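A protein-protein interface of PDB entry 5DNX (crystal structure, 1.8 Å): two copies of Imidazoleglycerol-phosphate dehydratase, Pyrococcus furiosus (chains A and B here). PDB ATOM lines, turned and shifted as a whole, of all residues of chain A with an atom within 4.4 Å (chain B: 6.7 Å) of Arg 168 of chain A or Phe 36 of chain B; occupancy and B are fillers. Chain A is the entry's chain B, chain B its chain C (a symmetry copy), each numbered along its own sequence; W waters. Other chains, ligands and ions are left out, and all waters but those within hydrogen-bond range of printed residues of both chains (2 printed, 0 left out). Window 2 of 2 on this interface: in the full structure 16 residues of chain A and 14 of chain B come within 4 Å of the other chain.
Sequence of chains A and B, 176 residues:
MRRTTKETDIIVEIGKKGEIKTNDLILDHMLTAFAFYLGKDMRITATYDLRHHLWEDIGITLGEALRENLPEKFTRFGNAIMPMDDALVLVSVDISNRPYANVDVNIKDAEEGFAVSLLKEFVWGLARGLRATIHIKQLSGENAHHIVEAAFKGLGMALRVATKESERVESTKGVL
NH2 of Arg 168 of chain A sits at hydrogen-bond distance from O of Phe 36 of chain B.
The side-chain hydroxyl of Ser 166 of chain A is in hydrogen-bond range of the backbone NH of Arg 168 of chain A, at 3.1 Å.
The side-chain hydroxyl (OG) of Ser 166 of chain A sits at hydrogen-bond distance from the side-chain carboxylate (OE2) of Glu 170 of chain A (2.7 Å).
NE of Arg 168 of chain A is in salt-bridge range of OE2 of Glu 170 of chain A (3.0 Å).
O of Tyr 37 of chain B is in hydrogen-bond range of NH2 of Arg 160 of chain B.
SD of Met 157 of chain B sits at hydrogen-bond distance from NH2 of Arg 160 of chain B (3.5 Å).
Among the printed residues, merely in contact across the chains: Val 169 of chain A with Phe 36 of chain B, Ser 171 of chain A with Phe 36 of chain B, Glu 170 of chain A with Tyr 37 of chain B, Thr 172 of chain A with Phe 36 of chain B, Glu 170 of chain A with Phe 36 of chain B, Arg 168 of chain A with Arg 160 of chain B, Thr 172 of chain A with Thr 32 of chain B and Thr 172 of chain A with Ala 33 of chain B.
Arg 168 of chain A touches just these residues of chain B: Phe 36 (2.9 Å) and Arg 160 (3.8 Å).
Phe 36 of chain B touches just these residues of chain A: Arg 168 (2.9 Å), Val 169 (3.3 Å), Glu 170 (3.7 Å), Ser 171 (3.4 Å) and Thr 172 (3.6 Å).
Printed residues of chain A within 4 Å of Tyr 37 of chain B: Glu 170.
Of the printed residues of chain B, Glu 170 of chain A touches Phe 36 and Tyr 37.
Printed residues of chain B within 4 Å of Val 169 of chain A: Phe 36 (3.3 Å).
Of the printed residues of chain A, Ala 33 of chain B touches Thr 172.
Of the printed residues of chain B, Ser 171 of chain A touches Phe 36 (3.4 Å).
Ala 35 of chain B touches none of the printed residues of chain A.
Met 157 of chain B touches none of the printed residues of chain A.
The nearest printed residue of chain A that does not touch Phe 36 of chain B is Ser 166 of chain A (7.3 Å).
Of the 15 printed residues of chain B, 5 touch a printed residue of chain A.
Hydrophobic or aromatic side chains of chain B within 4 Å of the printed part of chain A: Phe 36 and Tyr 37.
Along chain B the printed residues that touch a printed residue of chain A span positions 32 to 160.
Among the printed residues, no Asp or Glu carboxylate lies within 4 Å of a Lys or Arg side-chain nitrogen of the other chain.
No position is printed for both chains.
Water W1 bridges OH of Tyr 37 of chain B (2.7 Å) and N of Thr 172 of chain A (3.0 Å).
Water W2 lies within hydrogen-bond range of NH2 of Arg 160 of chain B (2.9 Å) and OE1 of Glu 170 of chain A (2.9 Å).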
ATOM      1  N   LYS A  73      39.556  10.532   1.912  1.00  0.00           N
ATOM      2  CA  LYS A  73      38.187  11.025   1.892  1.00  0.00           C
ATOM      3  C   LYS A  73      37.768  11.303   3.325  1.00  0.00           C
ATOM      4  O   LYS A  73      37.743  10.403   4.166  1.00  0.00           O
ATOM      5  CB  LYS A  73      37.267   9.980   1.258  1.00  0.00           C
ATOM      6  CG  LYS A  73      37.552   9.777  -0.221  1.00  0.00           C
ATOM      7  CD  LYS A  73      36.719   8.636  -0.765  1.00  0.00           C
ATOM      8  CE  LYS A  73      36.966   8.443  -2.246  1.00  0.00           C
ATOM      9  NZ  LYS A  73      36.318   7.166  -2.648  1.00  0.00           N
ATOM     10  N   SER A 166      35.321   9.640   5.373  1.00  0.00           N
ATOM     11  CA  SER A 166      34.041   9.678   4.665  1.00  0.00           C
ATOM     12  C   SER A 166      34.077   8.642   3.569  1.00  0.00           C
ATOM     13  O   SER A 166      35.154   8.310   3.057  1.00  0.00           O
ATOM     14  CB  SER A 166      33.805  11.039   4.003  1.00  0.00           C
ATOM     15  OG  SER A 166      32.612  11.055   3.211  1.00  0.00           O
ATOM     16  N   GLU A 167      32.892   8.238   3.098  1.00  0.00           N
ATOM     17  CA  GLU A 167      32.837   7.357   1.930  1.00  0.00           C
ATOM     18  C   GLU A 167      33.039   8.068   0.599  1.00  0.00           C
ATOM     19  O   GLU A 167      33.245   7.411  -0.415  1.00  0.00           O
ATOM     20  CB  GLU A 167      31.520   6.570   1.911  1.00  0.00           C
ATOM     21  CG  GLU A 167      31.377   5.587   3.069  1.00  0.00           C
ATOM     22  CD  GLU A 167      30.381   4.467   2.777  1.00  0.00           C
ATOM     23  OE1 GLU A 167      29.279   4.754   2.262  1.00  0.00           O
ATOM     24  OE2 GLU A 167      30.696   3.291   3.061  1.00  0.00           O
ATOM     25  N   ARG A 168      32.980   9.400   0.582  1.00  0.00           N
ATOM     26  CA  ARG A 168      33.059  10.157  -0.666  1.00  0.00           C
ATOM     27  C   ARG A 168      33.934  11.389  -0.513  1.00  0.00           C
ATOM     28  O   ARG A 168      34.227  11.802   0.596  1.00  0.00           O
ATOM     29  CB  ARG A 168      31.662  10.590  -1.117  1.00  0.00           C
ATOM     30  CG  ARG A 168      30.922  11.410  -0.078  1.00  0.00           C
ATOM     31  CD  ARG A 168      29.525  11.850  -0.504  1.00  0.00           C
ATOM     32  NE  ARG A 168      29.017  12.777   0.492  1.00  0.00           N
ATOM     33  CZ  ARG A 168      27.844  13.403   0.440  1.00  0.00           C
ATOM     34  NH1 ARG A 168      27.520  14.253   1.428  1.00  0.00           N
ATOM     35  NH2 ARG A 168      27.009  13.199  -0.572  1.00  0.00           N
ATOM     36  N   VAL A 169      34.304  11.969  -1.650  1.00  0.00           N
ATOM     37  CA  VAL A 169      34.902  13.311  -1.712  1.00  0.00           C
ATOM     38  C   VAL A 169      33.767  14.291  -1.367  1.00  0.00           C
ATOM     39  O   VAL A 169      32.763  14.368  -2.084  1.00  0.00           O
ATOM     40  CB  VAL A 169      35.501  13.609  -3.107  1.00  0.00           C
ATOM     41  CG1 VAL A 169      36.002  15.047  -3.185  1.00  0.00           C
ATOM     42  CG2 VAL A 169      36.661  12.641  -3.410  1.00  0.00           C
ATOM     43  N   GLU A 170      33.915  15.041  -0.276  1.00  0.00           N
ATOM     44  CA  GLU A 170      32.796  15.815   0.249  1.00  0.00           C
ATOM     45  C   GLU A 170      32.740  17.191  -0.404  1.00  0.00           C
ATOM     46  O   GLU A 170      32.976  18.201   0.258  1.00  0.00           O
ATOM     47  CB  GLU A 170      32.934  15.956   1.775  1.00  0.00           C
ATOM     48  CG  GLU A 170      32.667  14.675   2.543  1.00  0.00           C
ATOM     49  CD  GLU A 170      31.189  14.272   2.558  1.00  0.00           C
ATOM     50  OE1 GLU A 170      30.306  15.134   2.380  1.00  0.00           O
ATOM     51  OE2 GLU A 170      30.900  13.080   2.764  1.00  0.00           O
ATOM     52  N   SER A 171      32.491  17.211  -1.706  1.00  0.00           N
ATOM     53  CA  SER A 171      32.336  18.447  -2.465  1.00  0.00           C
ATOM     54  C   SER A 171      31.578  18.200  -3.737  1.00  0.00           C
ATOM     55  O   SER A 171      31.875  17.255  -4.479  1.00  0.00           O
ATOM     56  CB  SER A 171      33.672  19.117  -2.801  1.00  0.00           C
ATOM     57  OG  SER A 171      33.448  20.238  -3.672  1.00  0.00           O
ATOM     58  N   THR A 172      30.626  19.086  -4.023  1.00  0.00           N
ATOM     59  CA  THR A 172      29.848  18.989  -5.255  1.00  0.00           C
ATOM     60  C   THR A 172      30.703  19.252  -6.490  1.00  0.00           C
ATOM     61  O   THR A 172      30.304  18.893  -7.584  1.00  0.00           O
ATOM     62  CB  THR A 172      28.684  19.970  -5.306  1.00  0.00           C
ATOM     63  OG1 THR A 172      29.167  21.316  -5.129  1.00  0.00           O
ATOM     64  CG2 THR A 172      27.647  19.629  -4.254  1.00  0.00           C
ATOM     65  N   ILE B  20      20.151  17.382 -12.348  1.00  0.00           N
ATOM     66  CA  ILE B  20      19.300  18.479 -11.881  1.00  0.00           C
ATOM     67  C   ILE B  20      19.354  19.556 -12.963  1.00  0.00           C
ATOM     68  O   ILE B  20      20.402  20.208 -13.162  1.00  0.00           O
ATOM     69  CB  ILE B  20      19.791  18.955 -10.503  1.00  0.00           C
ATOM     70  CG1 ILE B  20      19.584  17.826  -9.486  1.00  0.00           C
ATOM     71  CG2 ILE B  20      19.089  20.240 -10.117  1.00  0.00           C
ATOM     72  CD1 ILE B  20      20.257  18.025  -8.150  1.00  0.00           C
ATOM     73  N   LEU B  31      20.448  23.451  -5.801  1.00  0.00           N
ATOM     74  CA  LEU B  31      19.819  22.154  -5.607  1.00  0.00           C
ATOM     75  C   LEU B  31      20.802  21.009  -5.581  1.00  0.00           C
ATOM     76  O   LEU B  31      20.586  20.050  -4.867  1.00  0.00           O
ATOM     77  CB  LEU B  31      18.770  21.904  -6.655  1.00  0.00           C
ATOM     78  CG  LEU B  31      17.530  22.792  -6.574  1.00  0.00           C
ATOM     79  CD1 LEU B  31      16.665  22.559  -7.783  1.00  0.00           C
ATOM     80  CD2 LEU B  31      16.758  22.583  -5.280  1.00  0.00           C
ATOM     81  N   THR B  32      21.875  21.111  -6.350  1.00  0.00           N
ATOM     82  CA  THR B  32      22.945  20.127  -6.319  1.00  0.00           C
ATOM     83  C   THR B  32      23.582  20.090  -4.921  1.00  0.00           C
ATOM     84  O   THR B  32      23.787  19.015  -4.359  1.00  0.00           O
ATOM     85  CB  THR B  32      23.971  20.429  -7.423  1.00  0.00           C
ATOM     86  OG1 THR B  32      23.333  20.333  -8.712  1.00  0.00           O
ATOM     87  CG2 THR B  32      25.149  19.493  -7.371  1.00  0.00           C
ATOM     88  N   ALA B  33      23.886  21.267  -4.382  1.00  0.00           N
ATOM     89  CA  ALA B  33      24.364  21.389  -3.005  1.00  0.00           C
ATOM     90  C   ALA B  33      23.367  20.784  -2.010  1.00  0.00           C
ATOM     91  O   ALA B  33      23.753  20.008  -1.151  1.00  0.00           O
ATOM     92  CB  ALA B  33      24.664  22.837  -2.663  1.00  0.00           C
ATOM     93  N   PHE B  34      22.091  21.149  -2.127  1.00  0.00           N
ATOM     94  CA  PHE B  34      21.081  20.625  -1.230  1.00  0.00           C
ATOM     95  C   PHE B  34      21.071  19.067  -1.245  1.00  0.00           C
ATOM     96  O   PHE B  34      21.138  18.430  -0.211  1.00  0.00           O
ATOM     97  CB  PHE B  34      19.710  21.161  -1.623  1.00  0.00           C
ATOM     98  CG  PHE B  34      18.597  20.552  -0.816  1.00  0.00           C
ATOM     99  CD1 PHE B  34      18.270  21.042   0.430  1.00  0.00           C
ATOM    100  CD2 PHE B  34      17.938  19.411  -1.285  1.00  0.00           C
ATOM    101  CE1 PHE B  34      17.290  20.435   1.193  1.00  0.00           C
ATOM    102  CE2 PHE B  34      16.956  18.805  -0.531  1.00  0.00           C
ATOM    103  CZ  PHE B  34      16.630  19.310   0.704  1.00  0.00           C
ATOM    104  N   ALA B  35      20.982  18.480  -2.446  1.00  0.00           N
ATOM    105  CA  ALA B  35      20.903  17.019  -2.602  1.00  0.00           C
ATOM    106  C   ALA B  35      22.153  16.326  -2.081  1.00  0.00           C
ATOM    107  O   ALA B  35      22.067  15.310  -1.393  1.00  0.00           O
ATOM    108  CB  ALA B  35      20.682  16.656  -4.048  1.00  0.00           C
ATOM    109  N   PHE B  36      23.309  16.927  -2.353  1.00  0.00           N
ATOM    110  CA  PHE B  36      24.594  16.348  -1.935  1.00  0.00           C
ATOM    111  C   PHE B  36      24.692  16.256  -0.405  1.00  0.00           C
ATOM    112  O   PHE B  36      25.096  15.228   0.137  1.00  0.00           O
ATOM    113  CB  PHE B  36      25.743  17.152  -2.526  1.00  0.00           C
ATOM    114  CG  PHE B  36      27.098  16.540  -2.304  1.00  0.00           C
ATOM    115  CD1 PHE B  36      27.624  15.661  -3.224  1.00  0.00           C
ATOM    116  CD2 PHE B  36      27.836  16.835  -1.164  1.00  0.00           C
ATOM    117  CE1 PHE B  36      28.871  15.085  -3.016  1.00  0.00           C
ATOM    118  CE2 PHE B  36      29.087  16.260  -0.939  1.00  0.00           C
ATOM    119  CZ  PHE B  36      29.606  15.401  -1.883  1.00  0.00           C
ATOM    120  N   TYR B  37      24.314  17.316   0.286  1.00  0.00           N
ATOM    121  CA  TYR B  37      24.367  17.333   1.750  1.00  0.00           C
ATOM    122  C   TYR B  37      23.200  16.613   2.413  1.00  0.00           C
ATOM    123  O   TYR B  37      23.339  16.113   3.535  1.00  0.00           O
ATOM    124  CB  TYR B  37      24.615  18.776   2.264  1.00  0.00           C
ATOM    125  CG  TYR B  37      26.024  19.166   1.852  1.00  0.00           C
ATOM    126  CD1 TYR B  37      27.126  18.558   2.466  1.00  0.00           C
ATOM    127  CD2 TYR B  37      26.265  19.976   0.734  1.00  0.00           C
ATOM    128  CE1 TYR B  37      28.427  18.809   2.021  1.00  0.00           C
ATOM    129  CE2 TYR B  37      27.565  20.249   0.304  1.00  0.00           C
ATOM    130  CZ  TYR B  37      28.641  19.696   0.970  1.00  0.00           C
ATOM    131  OH  TYR B  37      29.922  19.934   0.517  1.00  0.00           O
ATOM    132  N   LEU B  38      22.068  16.523   1.713  1.00  0.00           N
ATOM    133  CA  LEU B  38      20.991  15.642   2.141  1.00  0.00           C
ATOM    134  C   LEU B  38      21.471  14.200   2.103  1.00  0.00           C
ATOM    135  O   LEU B  38      21.046  13.401   2.922  1.00  0.00           O
ATOM    136  CB  LEU B  38      19.753  15.825   1.248  1.00  0.00           C
ATOM    137  CG  LEU B  38      18.526  14.966   1.612  1.00  0.00           C
ATOM    138  CD1 LEU B  38      17.940  15.338   2.962  1.00  0.00           C
ATOM    139  CD2 LEU B  38      17.477  15.093   0.523  1.00  0.00           C
ATOM    140  N   GLY B  39      22.341  13.887   1.148  1.00  0.00           N
ATOM    141  CA  GLY B  39      22.910  12.571   0.994  1.00  0.00           C
ATOM    142  C   GLY B  39      22.059  11.674   0.092  1.00  0.00           C
ATOM    143  O   GLY B  39      22.104  10.443   0.252  1.00  0.00           O
ATOM    144  N   LYS B  40      21.319  12.264  -0.852  1.00  0.00           N
ATOM    145  CA  LYS B  40      20.430  11.513  -1.769  1.00  0.00           C
ATOM    146  C   LYS B  40      20.699  11.912  -3.196  1.00  0.00           C
ATOM    147  O   LYS B  40      20.923  13.090  -3.501  1.00  0.00           O
ATOM    148  CB  LYS B  40      18.945  11.768  -1.441  1.00  0.00           C
ATOM    149  CG  LYS B  40      18.472  11.166  -0.139  1.00  0.00           C
ATOM    150  CD  LYS B  40      17.983   9.739  -0.305  1.00  0.00           C
ATOM    151  CE  LYS B  40      17.708   9.089   1.038  1.00  0.00           C
ATOM    152  NZ  LYS B  40      16.755   9.877   1.869  1.00  0.00           N
ATOM    153  N   MET B  42      19.101  12.684  -6.734  1.00  0.00           N
ATOM    154  CA  MET B  42      17.790  13.053  -7.208  1.00  0.00           C
ATOM    155  C   MET B  42      17.840  13.500  -8.646  1.00  0.00           C
ATOM    156  O   MET B  42      18.885  13.860  -9.180  1.00  0.00           O
ATOM    157  CB  MET B  42      17.046  14.054  -6.290  1.00  0.00           C
ATOM    158  CG  MET B  42      17.779  15.281  -5.844  1.00  0.00           C
ATOM    159  SD  MET B  42      16.806  16.317  -4.674  1.00  0.00           S
ATOM    160  CE  MET B  42      17.173  15.569  -3.098  1.00  0.00           C
ATOM    161  N   GLY B 156      20.271  20.932   3.342  1.00  0.00           N
ATOM    162  CA  GLY B 156      20.533  19.540   3.064  1.00  0.00           C
ATOM    163  C   GLY B 156      20.982  18.795   4.295  1.00  0.00           C
ATOM    164  O   GLY B 156      20.436  17.748   4.615  1.00  0.00           O
ATOM    165  N   MET B 157      21.981  19.333   5.008  1.00  0.00           N
ATOM    166  CA  MET B 157      22.481  18.696   6.231  1.00  0.00           C
ATOM    167  C   MET B 157      21.410  18.628   7.338  1.00  0.00           C
ATOM    168  O   MET B 157      21.305  17.607   8.036  1.00  0.00           O
ATOM    169  CB  MET B 157      23.724  19.442   6.750  1.00  0.00           C
ATOM    170  CG  MET B 157      24.427  18.807   7.925  1.00  0.00           C
ATOM    171  SD  MET B 157      25.363  17.383   7.384  1.00  0.00           S
ATOM    172  CE  MET B 157      26.697  18.209   6.504  1.00  0.00           C
ATOM    173  N   ARG B 160      18.888  16.017   6.404  1.00  0.00           N
ATOM    174  CA  ARG B 160      19.475  14.677   6.565  1.00  0.00           C
ATOM    175  C   ARG B 160      19.174  14.142   7.960  1.00  0.00           C
ATOM    176  O   ARG B 160      18.800  12.993   8.125  1.00  0.00           O
ATOM    177  CB  ARG B 160      20.990  14.682   6.322  1.00  0.00           C
ATOM    178  CG  ARG B 160      21.615  13.276   6.309  1.00  0.00           C
ATOM    179  CD  ARG B 160      23.128  13.278   6.517  1.00  0.00           C
ATOM    180  NE  ARG B 160      23.830  14.139   5.578  1.00  0.00           N
ATOM    181  CZ  ARG B 160      25.155  14.313   5.532  1.00  0.00           C
ATOM    182  NH1 ARG B 160      25.954  13.653   6.365  1.00  0.00           N
ATOM    183  NH2 ARG B 160      25.694  15.159   4.645  1.00  0.00           N
HETATM  184  O   HOH W   1      30.145  21.129  -1.885  1.00  0.00           O
HETATM  185  O   HOH W   2      28.426  15.991   4.385  1.00  0.00           O
